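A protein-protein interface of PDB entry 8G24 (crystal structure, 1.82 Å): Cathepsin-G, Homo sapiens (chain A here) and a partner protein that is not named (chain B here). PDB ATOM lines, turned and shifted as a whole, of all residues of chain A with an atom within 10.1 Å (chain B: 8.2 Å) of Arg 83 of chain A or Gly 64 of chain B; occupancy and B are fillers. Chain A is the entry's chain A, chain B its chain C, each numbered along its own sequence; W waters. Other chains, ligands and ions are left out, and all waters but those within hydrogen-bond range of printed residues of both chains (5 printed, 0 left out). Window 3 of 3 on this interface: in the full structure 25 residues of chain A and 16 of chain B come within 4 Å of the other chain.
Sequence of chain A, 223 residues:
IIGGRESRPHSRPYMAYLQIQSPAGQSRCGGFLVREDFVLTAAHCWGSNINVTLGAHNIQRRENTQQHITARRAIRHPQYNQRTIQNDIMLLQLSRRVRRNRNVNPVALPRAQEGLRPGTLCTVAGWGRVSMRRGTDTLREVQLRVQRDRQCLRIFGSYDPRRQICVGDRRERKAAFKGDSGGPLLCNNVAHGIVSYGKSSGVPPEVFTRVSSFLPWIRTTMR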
ATOM      1  N   HIS A  44      25.230 -13.549  25.082  1.00  0.00           N
ATOM      2  CA  HIS A  44      24.600 -14.385  26.100  1.00  0.00           C
ATOM      3  C   HIS A  44      23.630 -13.583  26.963  1.00  0.00           C
ATOM      4  O   HIS A  44      22.998 -14.167  27.841  1.00  0.00           O
ATOM      5  CB  HIS A  44      25.648 -15.093  26.975  1.00  0.00           C
ATOM      6  CG  HIS A  44      26.414 -14.173  27.875  1.00  0.00           C
ATOM      7  ND1 HIS A  44      27.673 -13.728  27.558  1.00  0.00           N
ATOM      8  CD2 HIS A  44      26.121 -13.637  29.089  1.00  0.00           C
ATOM      9  CE1 HIS A  44      28.127 -12.944  28.522  1.00  0.00           C
ATOM     10  NE2 HIS A  44      27.205 -12.871  29.465  1.00  0.00           N
ATOM     11  N   GLN A  79      26.884 -16.604  14.342  1.00  0.00           N
ATOM     12  CA  GLN A  79      27.663 -17.771  14.746  1.00  0.00           C
ATOM     13  C   GLN A  79      28.029 -17.729  16.228  1.00  0.00           C
ATOM     14  O   GLN A  79      29.000 -18.384  16.643  1.00  0.00           O
ATOM     15  CB  GLN A  79      28.921 -17.914  13.888  1.00  0.00           C
ATOM     16  CG  GLN A  79      28.701 -18.572  12.546  1.00  0.00           C
ATOM     17  CD  GLN A  79      28.035 -19.948  12.678  1.00  0.00           C
ATOM     18  OE1 GLN A  79      28.635 -20.902  13.181  1.00  0.00           O
ATOM     19  NE2 GLN A  79      26.807 -20.059  12.193  1.00  0.00           N
ATOM     20  N   TYR A  80      27.266 -16.964  17.036  1.00  0.00           N
ATOM     21  CA  TYR A  80      27.369 -17.053  18.487  1.00  0.00           C
ATOM     22  C   TYR A  80      27.354 -18.517  18.895  1.00  0.00           C
ATOM     23  O   TYR A  80      26.491 -19.288  18.452  1.00  0.00           O
ATOM     24  CB  TYR A  80      26.214 -16.297  19.182  1.00  0.00           C
ATOM     25  CG  TYR A  80      26.032 -16.601  20.647  1.00  0.00           C
ATOM     26  CD1 TYR A  80      27.074 -16.424  21.543  1.00  0.00           C
ATOM     27  CD2 TYR A  80      24.802 -17.066  21.146  1.00  0.00           C
ATOM     28  CE1 TYR A  80      26.916 -16.717  22.908  1.00  0.00           C
ATOM     29  CE2 TYR A  80      24.637 -17.344  22.526  1.00  0.00           C
ATOM     30  CZ  TYR A  80      25.713 -17.162  23.386  1.00  0.00           C
ATOM     31  OH  TYR A  80      25.584 -17.450  24.725  1.00  0.00           O
ATOM     32  N   ASN A  81      28.320 -18.895  19.739  1.00  0.00           N
ATOM     33  CA  ASN A  81      28.469 -20.268  20.235  1.00  0.00           C
ATOM     34  C   ASN A  81      28.207 -20.291  21.744  1.00  0.00           C
ATOM     35  O   ASN A  81      29.088 -19.937  22.545  1.00  0.00           O
ATOM     36  CB  ASN A  81      29.862 -20.823  19.899  1.00  0.00           C
ATOM     37  CG  ASN A  81      30.015 -22.275  20.263  1.00  0.00           C
ATOM     38  OD1 ASN A  81      29.421 -22.756  21.228  1.00  0.00           O
ATOM     39  ND2 ASN A  81      30.854 -22.985  19.509  1.00  0.00           N
ATOM     40  N   GLN A  82      26.997 -20.751  22.121  1.00  0.00           N
ATOM     41  CA  GLN A  82      26.595 -20.770  23.519  1.00  0.00           C
ATOM     42  C   GLN A  82      27.411 -21.750  24.357  1.00  0.00           C
ATOM     43  O   GLN A  82      27.486 -21.556  25.569  1.00  0.00           O
ATOM     44  CB  GLN A  82      25.083 -21.056  23.606  1.00  0.00           C
ATOM     45  CG  GLN A  82      24.659 -22.486  23.188  1.00  0.00           C
ATOM     46  CD  GLN A  82      24.456 -22.669  21.704  1.00  0.00           C
ATOM     47  OE1 GLN A  82      25.056 -21.955  20.875  1.00  0.00           O
ATOM     48  NE2 GLN A  82      23.600 -23.642  21.337  1.00  0.00           N
ATOM     49  N   ARG A  83      27.982 -22.800  23.753  1.00  0.00           N
ATOM     50  CA  ARG A  83      28.691 -23.796  24.528  1.00  0.00           C
ATOM     51  C   ARG A  83      30.017 -23.255  25.042  1.00  0.00           C
ATOM     52  O   ARG A  83      30.347 -23.448  26.214  1.00  0.00           O
ATOM     53  CB  ARG A  83      28.918 -25.026  23.672  1.00  0.00           C
ATOM     54  CG  ARG A  83      27.660 -25.837  23.337  1.00  0.00           C
ATOM     55  CD  ARG A  83      27.997 -27.173  22.679  1.00  0.00           C
ATOM     56  NE  ARG A  83      28.706 -26.976  21.421  1.00  0.00           N
ATOM     57  CZ  ARG A  83      28.104 -26.763  20.257  1.00  0.00           C
ATOM     58  NH1 ARG A  83      26.779 -26.757  20.150  1.00  0.00           N
ATOM     59  NH2 ARG A  83      28.846 -26.549  19.174  1.00  0.00           N
ATOM     60  N   THR A  84      30.770 -22.550  24.191  1.00  0.00           N
ATOM     61  CA  THR A  84      32.097 -22.031  24.516  1.00  0.00           C
ATOM     62  C   THR A  84      32.090 -20.528  24.766  1.00  0.00           C
ATOM     63  O   THR A  84      33.134 -19.970  25.125  1.00  0.00           O
ATOM     64  CB  THR A  84      33.083 -22.310  23.370  1.00  0.00           C
ATOM     65  OG1 THR A  84      32.572 -21.701  22.166  1.00  0.00           O
ATOM     66  CG2 THR A  84      33.222 -23.823  23.124  1.00  0.00           C
ATOM     67  N   ILE A  85      30.964 -19.857  24.527  1.00  0.00           N
ATOM     68  CA  ILE A  85      30.827 -18.402  24.641  1.00  0.00           C
ATOM     69  C   ILE A  85      31.822 -17.736  23.688  1.00  0.00           C
ATOM     70  O   ILE A  85      32.743 -17.013  24.111  1.00  0.00           O
ATOM     71  CB  ILE A  85      30.994 -17.906  26.084  1.00  0.00           C
ATOM     72  CG1 ILE A  85      30.228 -18.821  27.055  1.00  0.00           C
ATOM     73  CG2 ILE A  85      30.391 -16.506  26.218  1.00  0.00           C
ATOM     74  CD1 ILE A  85      30.128 -18.301  28.489  1.00  0.00           C
ATOM     75  N   GLN A  86      31.700 -18.059  22.408  1.00  0.00           N
ATOM     76  CA  GLN A  86      32.497 -17.462  21.344  1.00  0.00           C
ATOM     77  C   GLN A  86      31.578 -16.653  20.436  1.00  0.00           C
ATOM     78  O   GLN A  86      30.375 -16.876  20.400  1.00  0.00           O
ATOM     79  CB  GLN A  86      33.223 -18.508  20.527  1.00  0.00           C
ATOM     80  CG  GLN A  86      34.182 -17.927  19.513  1.00  0.00           C
ATOM     81  CD  GLN A  86      35.235 -17.048  20.160  1.00  0.00           C
ATOM     82  OE1 GLN A  86      35.105 -15.817  20.185  1.00  0.00           O
ATOM     83  NE2 GLN A  86      36.287 -17.675  20.689  1.00  0.00           N
ATOM     84  N   ASN A  87      32.143 -15.680  19.732  1.00  0.00           N
ATOM     85  CA  ASN A  87      31.345 -14.753  18.936  1.00  0.00           C
ATOM     86  C   ASN A  87      30.267 -14.116  19.808  1.00  0.00           C
ATOM     87  O   ASN A  87      29.109 -14.028  19.415  1.00  0.00           O
ATOM     88  CB  ASN A  87      30.720 -15.448  17.722  1.00  0.00           C
ATOM     89  CG  ASN A  87      31.763 -16.003  16.762  1.00  0.00           C
ATOM     90  OD1 ASN A  87      32.758 -15.348  16.460  1.00  0.00           O
ATOM     91  ND2 ASN A  87      31.526 -17.206  16.256  1.00  0.00           N
ATOM     92  N   ASP A  88      30.646 -13.742  21.023  1.00  0.00           N
ATOM     93  CA  ASP A  88      29.695 -13.340  22.063  1.00  0.00           C
ATOM     94  C   ASP A  88      29.468 -11.838  21.918  1.00  0.00           C
ATOM     95  O   ASP A  88      30.011 -11.019  22.669  1.00  0.00           O
ATOM     96  CB  ASP A  88      30.227 -13.718  23.439  1.00  0.00           C
ATOM     97  CG  ASP A  88      29.205 -13.450  24.560  1.00  0.00           C
ATOM     98  OD1 ASP A  88      27.999 -13.295  24.262  1.00  0.00           O
ATOM     99  OD2 ASP A  88      29.621 -13.398  25.718  1.00  0.00           O
ATOM    100  N   GLY A 157      40.059 -23.147  27.704  1.00  0.00           N
ATOM    101  CA  GLY A 157      40.507 -23.937  26.565  1.00  0.00           C
ATOM    102  C   GLY A 157      39.930 -23.502  25.230  1.00  0.00           C
ATOM    103  O   GLY A 157      40.469 -23.868  24.178  1.00  0.00           O
ATOM    104  N   SER A 158      38.848 -22.729  25.240  1.00  0.00           N
ATOM    105  CA  SER A 158      38.227 -22.268  24.008  1.00  0.00           C
ATOM    106  C   SER A 158      38.554 -20.814  23.697  1.00  0.00           C
ATOM    107  O   SER A 158      37.967 -20.237  22.773  1.00  0.00           O
ATOM    108  CB  SER A 158      36.711 -22.457  24.080  1.00  0.00           C
ATOM    109  OG  SER A 158      36.345 -23.801  23.833  1.00  0.00           O
ATOM    110  N   TYR A 159      39.474 -20.215  24.440  1.00  0.00           N
ATOM    111  CA  TYR A 159      39.885 -18.844  24.176  1.00  0.00           C
ATOM    112  C   TYR A 159      40.506 -18.727  22.791  1.00  0.00           C
ATOM    113  O   TYR A 159      41.323 -19.562  22.392  1.00  0.00           O
ATOM    114  CB  TYR A 159      40.879 -18.417  25.244  1.00  0.00           C
ATOM    115  CG  TYR A 159      41.424 -17.064  25.036  1.00  0.00           C
ATOM    116  CD1 TYR A 159      40.661 -15.931  25.305  1.00  0.00           C
ATOM    117  CD2 TYR A 159      42.725 -16.900  24.588  1.00  0.00           C
ATOM    118  CE1 TYR A 159      41.186 -14.676  25.116  1.00  0.00           C
ATOM    119  CE2 TYR A 159      43.259 -15.624  24.392  1.00  0.00           C
ATOM    120  CZ  TYR A 159      42.474 -14.524  24.658  1.00  0.00           C
ATOM    121  OH  TYR A 159      42.989 -13.268  24.454  1.00  0.00           O
ATOM    122  N   GLN A 164      38.995 -12.549  20.897  1.00  0.00           N
ATOM    123  CA  GLN A 164      38.835 -12.239  22.306  1.00  0.00           C
ATOM    124  C   GLN A 164      40.106 -11.627  22.873  1.00  0.00           C
ATOM    125  O   GLN A 164      41.203 -11.764  22.322  1.00  0.00           O
ATOM    126  CB  GLN A 164      38.483 -13.480  23.130  1.00  0.00           C
ATOM    127  CG  GLN A 164      37.025 -13.968  22.858  1.00  0.00           C
ATOM    128  CD  GLN A 164      36.862 -15.459  23.110  1.00  0.00           C
ATOM    129  OE1 GLN A 164      37.731 -16.271  22.781  1.00  0.00           O
ATOM    130  NE2 GLN A 164      35.744 -15.820  23.690  1.00  0.00           N
ATOM    131  N   SER A 196      32.603 -10.657  28.812  1.00  0.00           N
ATOM    132  CA  SER A 196      31.954 -11.905  28.399  1.00  0.00           C
ATOM    133  C   SER A 196      31.959 -12.944  29.514  1.00  0.00           C
ATOM    134  O   SER A 196      30.878 -13.316  30.002  1.00  0.00           O
ATOM    135  CB  SER A 196      32.646 -12.417  27.117  1.00  0.00           C
ATOM    136  OG  SER A 196      32.088 -13.619  26.635  1.00  0.00           O
ATOM    137  N   TYR A 197      33.128 -13.447  29.934  1.00  0.00           N
ATOM    138  CA  TYR A 197      33.099 -14.554  30.881  1.00  0.00           C
ATOM    139  C   TYR A 197      34.393 -14.639  31.681  1.00  0.00           C
ATOM    140  O   TYR A 197      35.385 -13.969  31.393  1.00  0.00           O
ATOM    141  CB  TYR A 197      32.828 -15.920  30.224  1.00  0.00           C
ATOM    142  CG  TYR A 197      33.920 -16.468  29.292  1.00  0.00           C
ATOM    143  CD1 TYR A 197      35.084 -17.046  29.801  1.00  0.00           C
ATOM    144  CD2 TYR A 197      33.761 -16.448  27.912  1.00  0.00           C
ATOM    145  CE1 TYR A 197      36.059 -17.548  28.968  1.00  0.00           C
ATOM    146  CE2 TYR A 197      34.724 -16.959  27.071  1.00  0.00           C
ATOM    147  CZ  TYR A 197      35.871 -17.520  27.586  1.00  0.00           C
ATOM    148  OH  TYR A 197      36.811 -18.065  26.739  1.00  0.00           O
ATOM    149  N   ILE B  25      25.758 -20.786  36.144  1.00  0.00           N
ATOM    150  CA  ILE B  25      26.179 -21.960  35.386  1.00  0.00           C
ATOM    151  C   ILE B  25      27.663 -21.831  35.069  1.00  0.00           C
ATOM    152  O   ILE B  25      28.096 -20.842  34.470  1.00  0.00           O
ATOM    153  CB  ILE B  25      25.392 -22.148  34.074  1.00  0.00           C
ATOM    154  CG1 ILE B  25      23.907 -22.367  34.343  1.00  0.00           C
ATOM    155  CG2 ILE B  25      25.949 -23.311  33.265  1.00  0.00           C
ATOM    156  CD1 ILE B  25      23.067 -22.336  33.088  1.00  0.00           C
ATOM    157  N   ALA B  26      28.434 -22.843  35.438  1.00  0.00           N
ATOM    158  CA  ALA B  26      29.818 -22.987  35.013  1.00  0.00           C
ATOM    159  C   ALA B  26      29.948 -24.298  34.249  1.00  0.00           C
ATOM    160  O   ALA B  26      29.523 -25.355  34.738  1.00  0.00           O
ATOM    161  CB  ALA B  26      30.778 -22.952  36.215  1.00  0.00           C
ATOM    162  N   VAL B  27      30.500 -24.224  33.039  1.00  0.00           N
ATOM    163  CA  VAL B  27      30.774 -25.406  32.228  1.00  0.00           C
ATOM    164  C   VAL B  27      32.240 -25.352  31.819  1.00  0.00           C
ATOM    165  O   VAL B  27      32.692 -24.372  31.210  1.00  0.00           O
ATOM    166  CB  VAL B  27      29.863 -25.503  30.985  1.00  0.00           C
ATOM    167  CG1 VAL B  27      30.250 -26.744  30.171  1.00  0.00           C
ATOM    168  CG2 VAL B  27      28.415 -25.513  31.353  1.00  0.00           C
ATOM    169  N   ASP B  28      32.978 -26.412  32.134  1.00  0.00           N
ATOM    170  CA  ASP B  28      34.389 -26.498  31.764  1.00  0.00           C
ATOM    171  C   ASP B  28      35.144 -25.253  32.223  1.00  0.00           C
ATOM    172  O   ASP B  28      35.954 -24.680  31.483  1.00  0.00           O
ATOM    173  CB  ASP B  28      34.545 -26.703  30.257  1.00  0.00           C
ATOM    174  CG  ASP B  28      34.157 -28.094  29.819  1.00  0.00           C
ATOM    175  OD1 ASP B  28      34.510 -29.065  30.522  1.00  0.00           O
ATOM    176  OD2 ASP B  28      33.490 -28.230  28.773  1.00  0.00           O
ATOM    177  N   ILE B  30      34.192 -22.209  32.663  1.00  0.00           N
ATOM    178  CA  ILE B  30      33.774 -20.953  32.060  1.00  0.00           C
ATOM    179  C   ILE B  30      32.393 -20.599  32.612  1.00  0.00           C
ATOM    180  O   ILE B  30      31.461 -21.419  32.558  1.00  0.00           O
ATOM    181  CB  ILE B  30      33.718 -21.067  30.526  1.00  0.00           C
ATOM    182  CG1 ILE B  30      35.074 -20.981  29.873  1.00  0.00           C
ATOM    183  CG2 ILE B  30      32.790 -19.978  29.969  1.00  0.00           C
ATOM    184  CD1 ILE B  30      35.060 -21.485  28.433  1.00  0.00           C
ATOM    185  N   LYS B  56      18.163 -28.957  33.728  1.00  0.00           N
ATOM    186  CA  LYS B  56      18.572 -29.486  32.435  1.00  0.00           C
ATOM    187  C   LYS B  56      18.142 -28.573  31.300  1.00  0.00           C
ATOM    188  O   LYS B  56      18.934 -28.297  30.397  1.00  0.00           O
ATOM    189  CB  LYS B  56      18.004 -30.885  32.254  1.00  0.00           C
ATOM    190  CG  LYS B  56      18.736 -31.883  33.125  1.00  0.00           C
ATOM    191  CD  LYS B  56      18.017 -33.198  33.289  1.00  0.00           C
ATOM    192  CE  LYS B  56      18.808 -34.024  34.287  1.00  0.00           C
ATOM    193  NZ  LYS B  56      18.274 -35.403  34.400  1.00  0.00           N
ATOM    194  N   ALA B  57      16.905 -28.066  31.347  1.00  0.00           N
ATOM    195  CA  ALA B  57      16.449 -27.148  30.310  1.00  0.00           C
ATOM    196  C   ALA B  57      17.326 -25.909  30.279  1.00  0.00           C
ATOM    197  O   ALA B  57      17.663 -25.402  29.204  1.00  0.00           O
ATOM    198  CB  ALA B  57      14.988 -26.764  30.555  1.00  0.00           C
ATOM    199  N   LEU B  58      17.683 -25.390  31.457  1.00  0.00           N
ATOM    200  CA  LEU B  58      18.522 -24.197  31.536  1.00  0.00           C
ATOM    201  C   LEU B  58      19.926 -24.483  31.009  1.00  0.00           C
ATOM    202  O   LEU B  58      20.483 -23.704  30.237  1.00  0.00           O
ATOM    203  CB  LEU B  58      18.577 -23.721  32.985  1.00  0.00           C
ATOM    204  CG  LEU B  58      18.788 -22.282  33.379  1.00  0.00           C
ATOM    205  CD1 LEU B  58      17.820 -21.314  32.774  1.00  0.00           C
ATOM    206  CD2 LEU B  58      18.643 -22.305  34.916  1.00  0.00           C
ATOM    207  N   LEU B  59      20.511 -25.600  31.416  1.00  0.00           N
ATOM    208  CA  LEU B  59      21.806 -25.992  30.892  1.00  0.00           C
ATOM    209  C   LEU B  59      21.780 -25.990  29.375  1.00  0.00           C
ATOM    210  O   LEU B  59      22.689 -25.432  28.744  1.00  0.00           O
ATOM    211  CB  LEU B  59      22.199 -27.358  31.451  1.00  0.00           C
ATOM    212  CG  LEU B  59      22.893 -27.287  32.817  1.00  0.00           C
ATOM    213  CD1 LEU B  59      22.991 -28.661  33.422  1.00  0.00           C
ATOM    214  CD2 LEU B  59      24.259 -26.625  32.686  1.00  0.00           C
ATOM    215  N   TYR B  60      20.727 -26.576  28.767  1.00  0.00           N
ATOM    216  CA  TYR B  60      20.688 -26.589  27.313  1.00  0.00           C
ATOM    217  C   TYR B  60      20.485 -25.187  26.724  1.00  0.00           C
ATOM    218  O   TYR B  60      21.204 -24.788  25.798  1.00  0.00           O
ATOM    219  CB  TYR B  60      19.621 -27.530  26.753  1.00  0.00           C
ATOM    220  CG  TYR B  60      19.671 -27.428  25.234  1.00  0.00           C
ATOM    221  CD1 TYR B  60      20.750 -27.931  24.526  1.00  0.00           C
ATOM    222  CD2 TYR B  60      18.673 -26.791  24.522  1.00  0.00           C
ATOM    223  CE1 TYR B  60      20.830 -27.833  23.153  1.00  0.00           C
ATOM    224  CE2 TYR B  60      18.723 -26.687  23.127  1.00  0.00           C
ATOM    225  CZ  TYR B  60      19.830 -27.211  22.444  1.00  0.00           C
ATOM    226  OH  TYR B  60      19.907 -27.109  21.094  1.00  0.00           O
ATOM    227  N   ASP B  61      19.462 -24.450  27.180  1.00  0.00           N
ATOM    228  CA  ASP B  61      19.109 -23.207  26.502  1.00  0.00           C
ATOM    229  C   ASP B  61      20.106 -22.091  26.794  1.00  0.00           C
ATOM    230  O   ASP B  61      20.205 -21.161  25.993  1.00  0.00           O
ATOM    231  CB  ASP B  61      17.681 -22.754  26.863  1.00  0.00           C
ATOM    232  CG  ASP B  61      17.221 -21.536  26.044  1.00  0.00           C
ATOM    233  OD1 ASP B  61      17.261 -21.563  24.776  1.00  0.00           O
ATOM    234  OD2 ASP B  61      16.761 -20.546  26.664  1.00  0.00           O
ATOM    235  N   GLU B  62      20.842 -22.141  27.917  1.00  0.00           N
ATOM    236  CA  GLU B  62      21.833 -21.100  28.175  1.00  0.00           C
ATOM    237  C   GLU B  62      23.235 -21.487  27.693  1.00  0.00           C
ATOM    238  O   GLU B  62      23.977 -20.630  27.212  1.00  0.00           O
ATOM    239  CB  GLU B  62      21.916 -20.774  29.669  1.00  0.00           C
ATOM    240  CG  GLU B  62      20.589 -20.299  30.319  1.00  0.00           C
ATOM    241  CD  GLU B  62      20.184 -18.907  29.926  1.00  0.00           C
ATOM    242  OE1 GLU B  62      21.021 -18.109  29.439  1.00  0.00           O
ATOM    243  OE2 GLU B  62      18.988 -18.575  30.099  1.00  0.00           O
ATOM    244  N   ARG B  63      23.629 -22.752  27.800  1.00  0.00           N
ATOM    245  CA  ARG B  63      24.995 -23.143  27.461  1.00  0.00           C
ATOM    246  C   ARG B  63      25.075 -24.336  26.512  1.00  0.00           C
ATOM    247  O   ARG B  63      26.170 -24.884  26.321  1.00  0.00           O
ATOM    248  CB  ARG B  63      25.784 -23.466  28.730  1.00  0.00           C
ATOM    249  CG  ARG B  63      26.168 -22.238  29.596  1.00  0.00           C
ATOM    250  CD  ARG B  63      26.967 -21.182  28.844  1.00  0.00           C
ATOM    251  NE  ARG B  63      28.294 -21.654  28.441  1.00  0.00           N
ATOM    252  CZ  ARG B  63      29.322 -21.831  29.262  1.00  0.00           C
ATOM    253  NH1 ARG B  63      29.213 -21.579  30.561  1.00  0.00           N
ATOM    254  NH2 ARG B  63      30.490 -22.268  28.764  1.00  0.00           N
ATOM    255  N   GLY B  64      23.966 -24.730  25.891  1.00  0.00           N
ATOM    256  CA  GLY B  64      23.991 -25.766  24.872  1.00  0.00           C
ATOM    257  C   GLY B  64      24.379 -27.142  25.387  1.00  0.00           C
ATOM    258  O   GLY B  64      24.749 -28.006  24.597  1.00  0.00           O
ATOM    259  N   VAL B  65      24.264 -27.370  26.687  1.00  0.00           N
ATOM    260  CA  VAL B  65      24.688 -28.611  27.327  1.00  0.00           C
ATOM    261  C   VAL B  65      23.572 -29.628  27.132  1.00  0.00           C
ATOM    262  O   VAL B  65      22.463 -29.447  27.649  1.00  0.00           O
ATOM    263  CB  VAL B  65      24.974 -28.381  28.818  1.00  0.00           C
ATOM    264  CG1 VAL B  65      25.131 -29.714  29.529  1.00  0.00           C
ATOM    265  CG2 VAL B  65      26.182 -27.469  29.023  1.00  0.00           C
ATOM    266  N   THR B  66      23.863 -30.709  26.413  1.00  0.00           N
ATOM    267  CA  THR B  66      22.842 -31.698  26.063  1.00  0.00           C
ATOM    268  C   THR B  66      22.743 -32.787  27.122  1.00  0.00           C
ATOM    269  O   THR B  66      23.628 -32.949  27.955  1.00  0.00           O
ATOM    270  CB  THR B  66      23.166 -32.356  24.721  1.00  0.00           C
ATOM    271  OG1 THR B  66      24.427 -33.019  24.843  1.00  0.00           O
ATOM    272  CG2 THR B  66      23.232 -31.329  23.592  1.00  0.00           C
ATOM    273  N   PRO B  67      21.673 -33.594  27.097  1.00  0.00           N
ATOM    274  CA  PRO B  67      21.644 -34.783  27.975  1.00  0.00           C
ATOM    275  C   PRO B  67      22.804 -35.737  27.758  1.00  0.00           C
ATOM    276  O   PRO B  67      23.342 -36.305  28.720  1.00  0.00           O
ATOM    277  CB  PRO B  67      20.310 -35.452  27.617  1.00  0.00           C
ATOM    278  CG  PRO B  67      19.439 -34.350  27.100  1.00  0.00           C
ATOM    279  CD  PRO B  67      20.370 -33.344  26.443  1.00  0.00           C
ATOM    280  N   LYS B  69      25.738 -34.928  26.825  1.00  0.00           N
ATOM    281  CA  LYS B  69      26.918 -34.298  27.414  1.00  0.00           C
ATOM    282  C   LYS B  69      26.949 -34.489  28.930  1.00  0.00           C
ATOM    283  O   LYS B  69      28.017 -34.717  29.512  1.00  0.00           O
ATOM    284  CB  LYS B  69      26.946 -32.813  27.044  1.00  0.00           C
ATOM    285  CG  LYS B  69      27.864 -31.958  27.859  1.00  0.00           C
ATOM    286  CD  LYS B  69      29.321 -32.178  27.522  1.00  0.00           C
ATOM    287  CE  LYS B  69      30.133 -30.914  27.756  1.00  0.00           C
ATOM    288  NZ  LYS B  69      29.977 -30.363  29.124  1.00  0.00           N
ATOM    289  N   ILE B  70      25.799 -34.381  29.593  1.00  0.00           N
ATOM    290  CA  ILE B  70      25.742 -34.684  31.025  1.00  0.00           C
ATOM    291  C   ILE B  70      26.111 -36.146  31.263  1.00  0.00           C
ATOM    292  O   ILE B  70      26.824 -36.480  32.222  1.00  0.00           O
ATOM    293  CB  ILE B  70      24.351 -34.316  31.578  1.00  0.00           C
ATOM    294  CG1 ILE B  70      24.240 -32.785  31.618  1.00  0.00           C
ATOM    295  CG2 ILE B  70      24.157 -34.917  32.965  1.00  0.00           C
ATOM    296  CD1 ILE B  70      22.832 -32.212  31.637  1.00  0.00           C
HETATM  297  O   HOH W   1      28.689 -25.933  27.501  1.00  0.00           O
HETATM  298  O   HOH W   2      32.836 -23.982  28.136  1.00  0.00           O
HETATM  299  O   HOH W   3      24.694 -27.816  21.769  1.00  0.00           O
HETATM  300  O   HOH W   4      23.409 -18.389  25.683  1.00  0.00           O
HETATM  301  O   HOH W   5      21.315 -24.162  22.965  1.00  0.00           O
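O of Gln 82 of chain A lies within hydrogen-bond range of NE of Arg 63 of chain B, 3.0 Å away. O of Arg 83 of chain A sits at hydrogen-bond distance from NH2 of Arg 63 of chain B (2.8 Å).
The side-chain amide oxygen (OD1) of Asn 81 of chain A is in hydrogen-bond range of the backbone NH (N) of Arg 83 of chain A (2.9 Å). The backbone carbonyl oxygen of Leu 59 of chain B sits at hydrogen-bond distance from the backbone NH of Gly 64 of chain B (3.2 Å). The backbone carbonyl oxygen (O) of Ile 85 of chain A is in hydrogen-bond range of the side-chain amide nitrogen (NE2) of Gln 164 of chain A (3.3 Å). O of Ile 30 of chain B sits at hydrogen-bond distance from NH1 of Arg 63 of chain B.
Among the printed residues, merely in contact across the chains: Gln 82 of chain A with Glu 62 of chain B, Gln 82 of chain A with Gly 64 of chain B, Arg 83 of chain A with Gly 64 of chain B, Ile 85 of chain A with Ile 30 of chain B, Ile 85 of chain A with Arg 63 of chain B and Tyr 197 of chain A with Ile 30 of chain B.
No residue of chain A comes within 4 Å of Tyr 60 of chain B. Printed residues of chain A within 4 Å of Arg 63 of chain B: Gln 82, Arg 83 and Ile 85. Of the printed residues of chain A, Glu 62 of chain B touches Gln 82 (3.8 Å). Of the printed residues of chain B, Gln 82 of chain A touches Glu 62 (3.8 Å), Arg 63 (3.0 Å) and Gly 64 (3.6 Å). Of the printed residues of chain B, Ile 85 of chain A touches Ile 30 (3.5 Å) and Arg 63 (3.7 Å). Printed residues of chain B within 4 Å of Tyr 197 of chain A: Ile 30 (3.7 Å). Printed residues of chain A within 4 Å of Ile 30 of chain B: Ile 85 and Tyr 197. Asp 28 of chain B touches none of the printed residues of chain A. Thr 66 of chain B touches none of the printed residues of chain A. The nearest residue of chain B that does not touch Arg 83 of chain A is Val 65 of chain B (5.0 Å). The nearest residue of chain A that does not touch Gly 64 of chain B is Asn 81 of chain A (7.2 Å).
Hydrophobic or aromatic side chains of chain B within 4 Å of the printed part of chain A: Ile 30. Hydrophobic or aromatic side chains of chain A that line the printed part of chain B: Ile 85 and Tyr 197. Among the printed residues, 8 pairs touch across the chains.
Water W4 lies within hydrogen-bond range of the side-chain hydroxyl (OH) of Tyr 80 of chain A (2.6 Å) and the backbone carbonyl oxygen (O) of Glu 62 of chain B (2.8 Å). Water W3 lies within hydrogen-bond range of the backbone carbonyl oxygen (O) of Gly 64 of chain B (2.8 Å) and the guanidinium group (NH1) of Arg 83 of chain A (2.8 Å). Water W5 lies within hydrogen-bond range of NE2 of Gln 82 of chain A (2.9 Å) and O of Tyr 60 of chain B (2.9 Å). Water W1 lies within hydrogen-bond range of the backbone carbonyl oxygen (O) of Arg 63 of chain B and the backbone carbonyl oxygen (O) of Arg 83 of chain A. Water W2 lies within hydrogen-bond range of NH2 of Arg 63 of chain B (3.0 Å), O of Val 27 of chain B (3.1 Å) and O of Arg 83 of chain A (3.2 Å).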
